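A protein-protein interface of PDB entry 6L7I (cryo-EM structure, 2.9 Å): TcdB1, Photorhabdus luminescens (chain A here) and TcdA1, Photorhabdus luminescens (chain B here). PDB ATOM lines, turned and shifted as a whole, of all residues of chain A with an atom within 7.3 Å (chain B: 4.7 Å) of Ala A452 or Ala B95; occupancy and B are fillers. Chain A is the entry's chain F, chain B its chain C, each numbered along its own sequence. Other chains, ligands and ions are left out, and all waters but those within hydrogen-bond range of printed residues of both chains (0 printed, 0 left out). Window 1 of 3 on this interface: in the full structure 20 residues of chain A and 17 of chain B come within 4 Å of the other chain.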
ATOM      1  N   ARG A 420      -6.518   1.824 -15.069  1.00  0.00           N
ATOM      2  CA  ARG A 420      -6.704   1.801 -16.514  1.00  0.00           C
ATOM      3  C   ARG A 420      -5.510   1.212 -17.249  1.00  0.00           C
ATOM      4  O   ARG A 420      -5.597   0.975 -18.455  1.00  0.00           O
ATOM      5  CB  ARG A 420      -6.978   3.211 -17.035  1.00  0.00           C
ATOM      6  CG  ARG A 420      -7.917   3.264 -18.226  1.00  0.00           C
ATOM      7  CD  ARG A 420      -7.690   4.532 -19.024  1.00  0.00           C
ATOM      8  NE  ARG A 420      -6.299   4.653 -19.447  1.00  0.00           N
ATOM      9  CZ  ARG A 420      -5.843   5.600 -20.256  1.00  0.00           C
ATOM     10  NH1 ARG A 420      -4.561   5.632 -20.583  1.00  0.00           N
ATOM     11  NH2 ARG A 420      -6.669   6.517 -20.740  1.00  0.00           N
ATOM     12  N   ASN A 421      -4.398   0.974 -16.565  1.00  0.00           N
ATOM     13  CA  ASN A 421      -3.218   0.421 -17.213  1.00  0.00           C
ATOM     14  C   ASN A 421      -2.868  -0.968 -16.696  1.00  0.00           C
ATOM     15  O   ASN A 421      -2.582  -1.868 -17.487  1.00  0.00           O
ATOM     16  CB  ASN A 421      -2.025   1.361 -17.026  1.00  0.00           C
ATOM     17  CG  ASN A 421      -2.394   2.821 -17.183  1.00  0.00           C
ATOM     18  OD1 ASN A 421      -2.369   3.366 -18.286  1.00  0.00           O
ATOM     19  ND2 ASN A 421      -2.718   3.470 -16.072  1.00  0.00           N
ATOM     20  N   TRP A 423      -3.694  -4.182 -13.591  1.00  0.00           N
ATOM     21  CA  TRP A 423      -4.619  -4.777 -12.642  1.00  0.00           C
ATOM     22  C   TRP A 423      -3.832  -5.433 -11.525  1.00  0.00           C
ATOM     23  O   TRP A 423      -2.801  -6.061 -11.770  1.00  0.00           O
ATOM     24  CB  TRP A 423      -5.506  -5.824 -13.306  1.00  0.00           C
ATOM     25  CG  TRP A 423      -6.529  -5.290 -14.224  1.00  0.00           C
ATOM     26  CD1 TRP A 423      -6.646  -4.016 -14.670  1.00  0.00           C
ATOM     27  CD2 TRP A 423      -7.588  -6.027 -14.829  1.00  0.00           C
ATOM     28  NE1 TRP A 423      -7.718  -3.906 -15.510  1.00  0.00           N
ATOM     29  CE2 TRP A 423      -8.314  -5.131 -15.626  1.00  0.00           C
ATOM     30  CE3 TRP A 423      -7.997  -7.358 -14.769  1.00  0.00           C
ATOM     31  CZ2 TRP A 423      -9.419  -5.523 -16.362  1.00  0.00           C
ATOM     32  CZ3 TRP A 423      -9.097  -7.741 -15.498  1.00  0.00           C
ATOM     33  CH2 TRP A 423      -9.793  -6.830 -16.285  1.00  0.00           C
ATOM     34  N   ILE A 449      -0.700  -9.650 -17.937  1.00  0.00           N
ATOM     35  CA  ILE A 449      -1.390  -9.259 -19.164  1.00  0.00           C
ATOM     36  C   ILE A 449      -2.802  -8.812 -18.822  1.00  0.00           C
ATOM     37  O   ILE A 449      -3.430  -9.341 -17.902  1.00  0.00           O
ATOM     38  CB  ILE A 449      -1.416 -10.395 -20.206  1.00  0.00           C
ATOM     39  CG1 ILE A 449      -1.892 -11.702 -19.562  1.00  0.00           C
ATOM     40  CG2 ILE A 449      -0.081 -10.526 -20.907  1.00  0.00           C
ATOM     41  CD1 ILE A 449      -2.170 -12.803 -20.543  1.00  0.00           C
ATOM     42  N   THR A 450      -3.288  -7.820 -19.554  1.00  0.00           N
ATOM     43  CA  THR A 450      -4.623  -7.264 -19.407  1.00  0.00           C
ATOM     44  C   THR A 450      -5.173  -6.997 -20.799  1.00  0.00           C
ATOM     45  O   THR A 450      -4.402  -6.696 -21.716  1.00  0.00           O
ATOM     46  CB  THR A 450      -4.604  -5.971 -18.571  1.00  0.00           C
ATOM     47  OG1 THR A 450      -3.462  -5.182 -18.919  1.00  0.00           O
ATOM     48  CG2 THR A 450      -4.574  -6.290 -17.084  1.00  0.00           C
ATOM     49  N   PRO A 451      -6.494  -7.094 -20.993  1.00  0.00           N
ATOM     50  CA  PRO A 451      -7.046  -7.081 -22.357  1.00  0.00           C
ATOM     51  C   PRO A 451      -7.009  -5.745 -23.091  1.00  0.00           C
ATOM     52  O   PRO A 451      -7.680  -5.635 -24.122  1.00  0.00           O
ATOM     53  CB  PRO A 451      -8.500  -7.517 -22.144  1.00  0.00           C
ATOM     54  CG  PRO A 451      -8.500  -8.229 -20.879  1.00  0.00           C
ATOM     55  CD  PRO A 451      -7.512  -7.532 -20.024  1.00  0.00           C
ATOM     56  N   ALA A 452      -6.355  -4.705 -22.563  1.00  0.00           N
ATOM     57  CA  ALA A 452      -5.913  -3.514 -23.297  1.00  0.00           C
ATOM     58  C   ALA A 452      -7.007  -2.599 -23.843  1.00  0.00           C
ATOM     59  O   ALA A 452      -6.699  -1.522 -24.357  1.00  0.00           O
ATOM     60  CB  ALA A 452      -5.000  -3.911 -24.458  1.00  0.00           C
ATOM     61  N   VAL A 453      -8.273  -2.995 -23.748  1.00  0.00           N
ATOM     62  CA  VAL A 453      -9.378  -2.101 -24.066  1.00  0.00           C
ATOM     63  C   VAL A 453     -10.175  -1.922 -22.786  1.00  0.00           C
ATOM     64  O   VAL A 453     -11.075  -2.709 -22.485  1.00  0.00           O
ATOM     65  CB  VAL A 453     -10.259  -2.638 -25.205  1.00  0.00           C
ATOM     66  CG1 VAL A 453     -11.168  -1.547 -25.713  1.00  0.00           C
ATOM     67  CG2 VAL A 453      -9.415  -3.172 -26.335  1.00  0.00           C
ATOM     68  N   GLN A 454      -9.843  -0.891 -22.024  1.00  0.00           N
ATOM     69  CA  GLN A 454     -10.380  -0.705 -20.690  1.00  0.00           C
ATOM     70  C   GLN A 454     -11.656   0.119 -20.662  1.00  0.00           C
ATOM     71  O   GLN A 454     -12.197   0.354 -19.578  1.00  0.00           O
ATOM     72  CB  GLN A 454      -9.329  -0.039 -19.807  1.00  0.00           C
ATOM     73  CG  GLN A 454      -8.018  -0.789 -19.731  1.00  0.00           C
ATOM     74  CD  GLN A 454      -8.119  -2.057 -18.929  1.00  0.00           C
ATOM     75  OE1 GLN A 454      -7.819  -3.143 -19.419  1.00  0.00           O
ATOM     76  NE2 GLN A 454      -8.557  -1.930 -17.688  1.00  0.00           N
ATOM     77  N   ASP A 455     -12.148   0.559 -21.815  1.00  0.00           N
ATOM     78  CA  ASP A 455     -13.322   1.412 -21.900  1.00  0.00           C
ATOM     79  C   ASP A 455     -14.517   0.605 -22.376  1.00  0.00           C
ATOM     80  O   ASP A 455     -14.376  -0.258 -23.250  1.00  0.00           O
ATOM     81  CB  ASP A 455     -13.082   2.584 -22.854  1.00  0.00           C
ATOM     82  CG  ASP A 455     -12.320   3.722 -22.206  1.00  0.00           C
ATOM     83  OD1 ASP A 455     -11.864   3.570 -21.052  1.00  0.00           O
ATOM     84  OD2 ASP A 455     -12.175   4.777 -22.857  1.00  0.00           O
ATOM     85  N   TRP A 470     -14.019 -10.463 -20.298  1.00  0.00           N
ATOM     86  CA  TRP A 470     -13.908  -9.009 -20.267  1.00  0.00           C
ATOM     87  C   TRP A 470     -14.667  -8.502 -21.487  1.00  0.00           C
ATOM     88  O   TRP A 470     -14.097  -8.306 -22.556  1.00  0.00           O
ATOM     89  CB  TRP A 470     -12.446  -8.590 -20.269  1.00  0.00           C
ATOM     90  CG  TRP A 470     -12.196  -7.125 -20.193  1.00  0.00           C
ATOM     91  CD1 TRP A 470     -11.647  -6.347 -21.160  1.00  0.00           C
ATOM     92  CD2 TRP A 470     -12.456  -6.262 -19.085  1.00  0.00           C
ATOM     93  NE1 TRP A 470     -11.555  -5.051 -20.731  1.00  0.00           N
ATOM     94  CE2 TRP A 470     -12.047  -4.973 -19.456  1.00  0.00           C
ATOM     95  CE3 TRP A 470     -13.004  -6.451 -17.820  1.00  0.00           C
ATOM     96  CZ2 TRP A 470     -12.167  -3.882 -18.608  1.00  0.00           C
ATOM     97  CZ3 TRP A 470     -13.123  -5.370 -16.982  1.00  0.00           C
ATOM     98  CH2 TRP A 470     -12.707  -4.103 -17.377  1.00  0.00           C
ATOM     99  N   ILE A 472     -16.139  -6.310 -23.948  1.00  0.00           N
ATOM    100  CA  ILE A 472     -15.981  -4.946 -24.433  1.00  0.00           C
ATOM    101  C   ILE A 472     -17.088  -4.677 -25.439  1.00  0.00           C
ATOM    102  O   ILE A 472     -17.043  -5.178 -26.560  1.00  0.00           O
ATOM    103  CB  ILE A 472     -14.604  -4.734 -25.069  1.00  0.00           C
ATOM    104  CG1 ILE A 472     -13.494  -5.095 -24.088  1.00  0.00           C
ATOM    105  CG2 ILE A 472     -14.459  -3.307 -25.523  1.00  0.00           C
ATOM    106  CD1 ILE A 472     -12.369  -5.855 -24.717  1.00  0.00           C
ATOM    107  N   HIS A 481     -12.649 -10.848 -24.187  1.00  0.00           N
ATOM    108  CA  HIS A 481     -11.485 -11.673 -23.897  1.00  0.00           C
ATOM    109  C   HIS A 481     -11.831 -12.560 -22.715  1.00  0.00           C
ATOM    110  O   HIS A 481     -12.323 -12.063 -21.702  1.00  0.00           O
ATOM    111  CB  HIS A 481     -10.263 -10.825 -23.539  1.00  0.00           C
ATOM    112  CG  HIS A 481      -9.812  -9.902 -24.622  1.00  0.00           C
ATOM    113  ND1 HIS A 481     -10.448  -8.714 -24.897  1.00  0.00           N
ATOM    114  CD2 HIS A 481      -8.768  -9.977 -25.475  1.00  0.00           C
ATOM    115  CE1 HIS A 481      -9.825  -8.104 -25.888  1.00  0.00           C
ATOM    116  NE2 HIS A 481      -8.802  -8.851 -26.258  1.00  0.00           N
ATOM    117  N   THR A 490      -7.481 -15.068 -23.188  1.00  0.00           N
ATOM    118  CA  THR A 490      -7.835 -15.356 -24.567  1.00  0.00           C
ATOM    119  C   THR A 490      -7.789 -14.050 -25.364  1.00  0.00           C
ATOM    120  O   THR A 490      -7.980 -12.965 -24.817  1.00  0.00           O
ATOM    121  CB  THR A 490      -9.227 -16.017 -24.583  1.00  0.00           C
ATOM    122  OG1 THR A 490      -9.159 -17.245 -23.856  1.00  0.00           O
ATOM    123  CG2 THR A 490      -9.742 -16.359 -25.975  1.00  0.00           C
ATOM    124  N   ARG A 491      -7.503 -14.146 -26.662  1.00  0.00           N
ATOM    125  CA  ARG A 491      -7.571 -12.980 -27.531  1.00  0.00           C
ATOM    126  C   ARG A 491      -9.022 -12.547 -27.749  1.00  0.00           C
ATOM    127  O   ARG A 491      -9.973 -13.142 -27.232  1.00  0.00           O
ATOM    128  CB  ARG A 491      -6.902 -13.268 -28.866  1.00  0.00           C
ATOM    129  CG  ARG A 491      -5.523 -13.835 -28.721  1.00  0.00           C
ATOM    130  CD  ARG A 491      -4.786 -13.796 -30.024  1.00  0.00           C
ATOM    131  NE  ARG A 491      -3.782 -14.846 -30.095  1.00  0.00           N
ATOM    132  CZ  ARG A 491      -2.922 -14.979 -31.095  1.00  0.00           C
ATOM    133  NH1 ARG A 491      -2.944 -14.124 -32.107  1.00  0.00           N
ATOM    134  NH2 ARG A 491      -2.043 -15.969 -31.080  1.00  0.00           N
ATOM    135  N   PHE A 492      -9.184 -11.491 -28.540  1.00  0.00           N
ATOM    136  CA  PHE A 492     -10.485 -10.866 -28.739  1.00  0.00           C
ATOM    137  C   PHE A 492     -11.405 -11.788 -29.529  1.00  0.00           C
ATOM    138  O   PHE A 492     -11.108 -12.142 -30.674  1.00  0.00           O
ATOM    139  CB  PHE A 492     -10.307  -9.534 -29.459  1.00  0.00           C
ATOM    140  CG  PHE A 492     -11.570  -8.747 -29.603  1.00  0.00           C
ATOM    141  CD1 PHE A 492     -12.121  -8.095 -28.519  1.00  0.00           C
ATOM    142  CD2 PHE A 492     -12.199  -8.648 -30.826  1.00  0.00           C
ATOM    143  CE1 PHE A 492     -13.273  -7.370 -28.649  1.00  0.00           C
ATOM    144  CE2 PHE A 492     -13.357  -7.925 -30.964  1.00  0.00           C
ATOM    145  CZ  PHE A 492     -13.894  -7.289 -29.875  1.00  0.00           C
ATOM    146  N   LEU B  93      -7.416  -0.967 -31.293  1.00  0.00           N
ATOM    147  CA  LEU B  93      -6.600  -2.169 -31.451  1.00  0.00           C
ATOM    148  C   LEU B  93      -6.874  -3.125 -30.303  1.00  0.00           C
ATOM    149  O   LEU B  93      -6.339  -2.936 -29.198  1.00  0.00           O
ATOM    150  CB  LEU B  93      -5.121  -1.803 -31.501  1.00  0.00           C
ATOM    151  CG  LEU B  93      -4.723  -0.974 -32.714  1.00  0.00           C
ATOM    152  CD1 LEU B  93      -3.579  -0.079 -32.373  1.00  0.00           C
ATOM    153  CD2 LEU B  93      -4.345  -1.877 -33.845  1.00  0.00           C
ATOM    154  N   PRO B  94      -7.694  -4.153 -30.498  1.00  0.00           N
ATOM    155  CA  PRO B  94      -7.944  -5.100 -29.409  1.00  0.00           C
ATOM    156  C   PRO B  94      -6.795  -6.076 -29.254  1.00  0.00           C
ATOM    157  O   PRO B  94      -6.657  -7.017 -30.040  1.00  0.00           O
ATOM    158  CB  PRO B  94      -9.229  -5.812 -29.840  1.00  0.00           C
ATOM    159  CG  PRO B  94      -9.458  -5.432 -31.254  1.00  0.00           C
ATOM    160  CD  PRO B  94      -8.367  -4.555 -31.737  1.00  0.00           C
ATOM    161  N   ALA B  95      -5.972  -5.868 -28.235  1.00  0.00           N
ATOM    162  CA  ALA B  95      -4.794  -6.685 -28.021  1.00  0.00           C
ATOM    163  C   ALA B  95      -4.746  -7.080 -26.559  1.00  0.00           C
ATOM    164  O   ALA B  95      -5.687  -6.846 -25.802  1.00  0.00           O
ATOM    165  CB  ALA B  95      -3.518  -5.945 -28.421  1.00  0.00           C
ATOM    166  N   LEU B  96      -3.645  -7.705 -26.171  1.00  0.00           N
ATOM    167  CA  LEU B  96      -3.353  -7.992 -24.776  1.00  0.00           C
ATOM    168  C   LEU B  96      -2.047  -7.305 -24.428  1.00  0.00           C
ATOM    169  O   LEU B  96      -0.983  -7.709 -24.907  1.00  0.00           O
ATOM    170  CB  LEU B  96      -3.258  -9.493 -24.527  1.00  0.00           C
ATOM    171  CG  LEU B  96      -4.452 -10.303 -25.007  1.00  0.00           C
ATOM    172  CD1 LEU B  96      -4.066 -11.744 -25.231  1.00  0.00           C
ATOM    173  CD2 LEU B  96      -5.549 -10.191 -23.987  1.00  0.00           C
ATOM    174  N   LEU B  97      -2.127  -6.268 -23.612  1.00  0.00           N
ATOM    175  CA  LEU B  97      -0.981  -5.443 -23.283  1.00  0.00           C
ATOM    176  C   LEU B  97      -0.343  -5.933 -21.994  1.00  0.00           C
ATOM    177  O   LEU B  97      -0.908  -6.743 -21.263  1.00  0.00           O
ATOM    178  CB  LEU B  97      -1.402  -3.978 -23.150  1.00  0.00           C
ATOM    179  CG  LEU B  97      -1.280  -3.162 -24.429  1.00  0.00           C
ATOM    180  CD1 LEU B  97      -1.931  -1.817 -24.248  1.00  0.00           C
ATOM    181  CD2 LEU B  97       0.174  -3.006 -24.786  1.00  0.00           C
ATOM    182  N   HIS B 126      -3.399   4.479 -27.032  1.00  0.00           N
ATOM    183  CA  HIS B 126      -4.022   3.454 -26.210  1.00  0.00           C
ATOM    184  C   HIS B 126      -4.949   2.523 -26.968  1.00  0.00           C
ATOM    185  O   HIS B 126      -5.171   1.401 -26.505  1.00  0.00           O
ATOM    186  CB  HIS B 126      -4.794   4.079 -25.036  1.00  0.00           C
ATOM    187  CG  HIS B 126      -5.780   5.127 -25.441  1.00  0.00           C
ATOM    188  ND1 HIS B 126      -5.524   6.474 -25.319  1.00  0.00           N
ATOM    189  CD2 HIS B 126      -7.030   5.027 -25.949  1.00  0.00           C
ATOM    190  CE1 HIS B 126      -6.570   7.160 -25.742  1.00  0.00           C
ATOM    191  NE2 HIS B 126      -7.497   6.305 -26.132  1.00  0.00           N
ATOM    192  N   MET B 128      -8.328   2.691 -27.797  1.00  0.00           N
ATOM    193  CA  MET B 128      -9.709   2.555 -27.337  1.00  0.00           C
ATOM    194  C   MET B 128     -10.460   3.733 -27.939  1.00  0.00           C
ATOM    195  O   MET B 128     -10.565   4.766 -27.274  1.00  0.00           O
ATOM    196  CB  MET B 128      -9.811   2.556 -25.816  1.00  0.00           C
ATOM    197  CG  MET B 128      -8.942   1.551 -25.105  1.00  0.00           C
ATOM    198  SD  MET B 128      -9.083   1.725 -23.323  1.00  0.00           S
ATOM    199  CE  MET B 128      -8.124   3.204 -23.046  1.00  0.00           C
ATOM    200  N   MET B 174       3.264  -7.505 -28.300  1.00  0.00           N
ATOM    201  CA  MET B 174       1.887  -7.027 -28.372  1.00  0.00           C
ATOM    202  C   MET B 174       1.233  -7.401 -29.691  1.00  0.00           C
ATOM    203  O   MET B 174       0.033  -7.678 -29.727  1.00  0.00           O
ATOM    204  CB  MET B 174       1.849  -5.513 -28.189  1.00  0.00           C
ATOM    205  CG  MET B 174       0.466  -4.936 -27.966  1.00  0.00           C
ATOM    206  SD  MET B 174      -0.324  -4.304 -29.461  1.00  0.00           S
ATOM    207  CE  MET B 174       0.950  -3.224 -30.090  1.00  0.00           C
ATOM    208  N   THR B 177      -0.462 -10.790 -29.892  1.00  0.00           N
ATOM    209  CA  THR B 177      -1.787 -10.864 -29.303  1.00  0.00           C
ATOM    210  C   THR B 177      -2.841 -10.136 -30.122  1.00  0.00           C
ATOM    211  O   THR B 177      -4.020 -10.190 -29.764  1.00  0.00           O
ATOM    212  CB  THR B 177      -1.757 -10.294 -27.890  1.00  0.00           C
ATOM    213  OG1 THR B 177      -1.461  -8.897 -27.950  1.00  0.00           O
ATOM    214  CG2 THR B 177      -0.689 -10.984 -27.070  1.00  0.00           C
ATOM    215  N   LEU B 178      -2.453  -9.472 -31.206  1.00  0.00           N
ATOM    216  CA  LEU B 178      -3.371  -8.678 -32.006  1.00  0.00           C
ATOM    217  C   LEU B 178      -4.102  -9.561 -33.004  1.00  0.00           C
ATOM    218  O   LEU B 178      -3.474 -10.260 -33.802  1.00  0.00           O
ATOM    219  CB  LEU B 178      -2.622  -7.565 -32.736  1.00  0.00           C
ATOM    220  CG  LEU B 178      -3.473  -6.444 -33.327  1.00  0.00           C
ATOM    221  CD1 LEU B 178      -4.420  -5.887 -32.296  1.00  0.00           C
ATOM    222  CD2 LEU B 178      -2.576  -5.353 -33.856  1.00  0.00           C
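Asn A421 touches none of the printed residues of chain B. Of the printed residues of chain B, Pro A451 touches Ala B95 and Leu B96. Printed residues of chain B within 4 Å of Asp A455: Met B128 (3.6 Å). Printed residues of chain B within 4 Å of Arg A491: Thr B177. Leu B93 touches none of the printed residues of chain A. Printed residues of chain A within 4 Å of Pro B94: Val A453 (3.9 Å) and Phe A492 (3.8 Å). Ala B95 touches three residues of chain A. Printed residues of chain A within 4 Å of Leu B96: Thr A450, Pro A451, His A481 and Thr A490. The nearest residue of chain B that does not touch Ala A452 is Leu B96 (4.4 Å).
N of Leu B97 lies within hydrogen-bond range of O of Thr A450. SD of Met B128 is in hydrogen-bond range of N of Gln A454 (3.0 Å). The side-chain sulfur (SD) of Met B128 is in hydrogen-bond range of the backbone NH (N) of Asp A455 (3.6 Å). O of Ala B95 sits close to O of Pro A451 (2.9 Å).
Among the printed residues, merely in contact across the chains: Ile A449 with Leu B97, Thr A450 with Leu B96, Pro A451 with Leu B96, Ala A452 with Ala B95, Ala A452 with Leu B97, Ala A452 with His B126, Ala A452 with Met B128, Val A453 with Pro B94, Val A453 with Met B128, His A481 with Ala B95, His A481 with Leu B96, Thr A490 with Leu B96, Arg A491 with Thr B177 and Phe A492 with Pro B94.
The side-chain hydroxyl (OG1) of Thr B177 is in hydrogen-bond range of the backbone NH (N) of Leu B96. The backbone carbonyl oxygen (O) of Met B174 lies within hydrogen-bond range of the side-chain hydroxyl (OG1) of Thr B177 (2.6 Å). NE1 of Trp A423 sits close to NE2 of Gln A454 (3.1 Å). O of Val A453 lies within hydrogen-bond range of NE1 of Trp A470, 3.0 Å away. The backbone NH (N) of Trp A470 lies within hydrogen-bond range of the backbone carbonyl oxygen (O) of His A481, at 2.7 Å.
Printed residues of chain A that touch a printed residue of chain B: Ile A449, Thr A450, Pro A451, Ala A452, Val A453, Gln A454, Asp A455, His A481, Thr A490, Arg A491 and Phe A492. Hydrophobic or aromatic side chains of chain B that line the printed part of chain A: Pro B94, Leu B96, Leu B97 and Met B128. Among the printed residues, no Asp or Glu carboxylate lies within 4 Å of a Lys or Arg side-chain nitrogen of the other chain.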
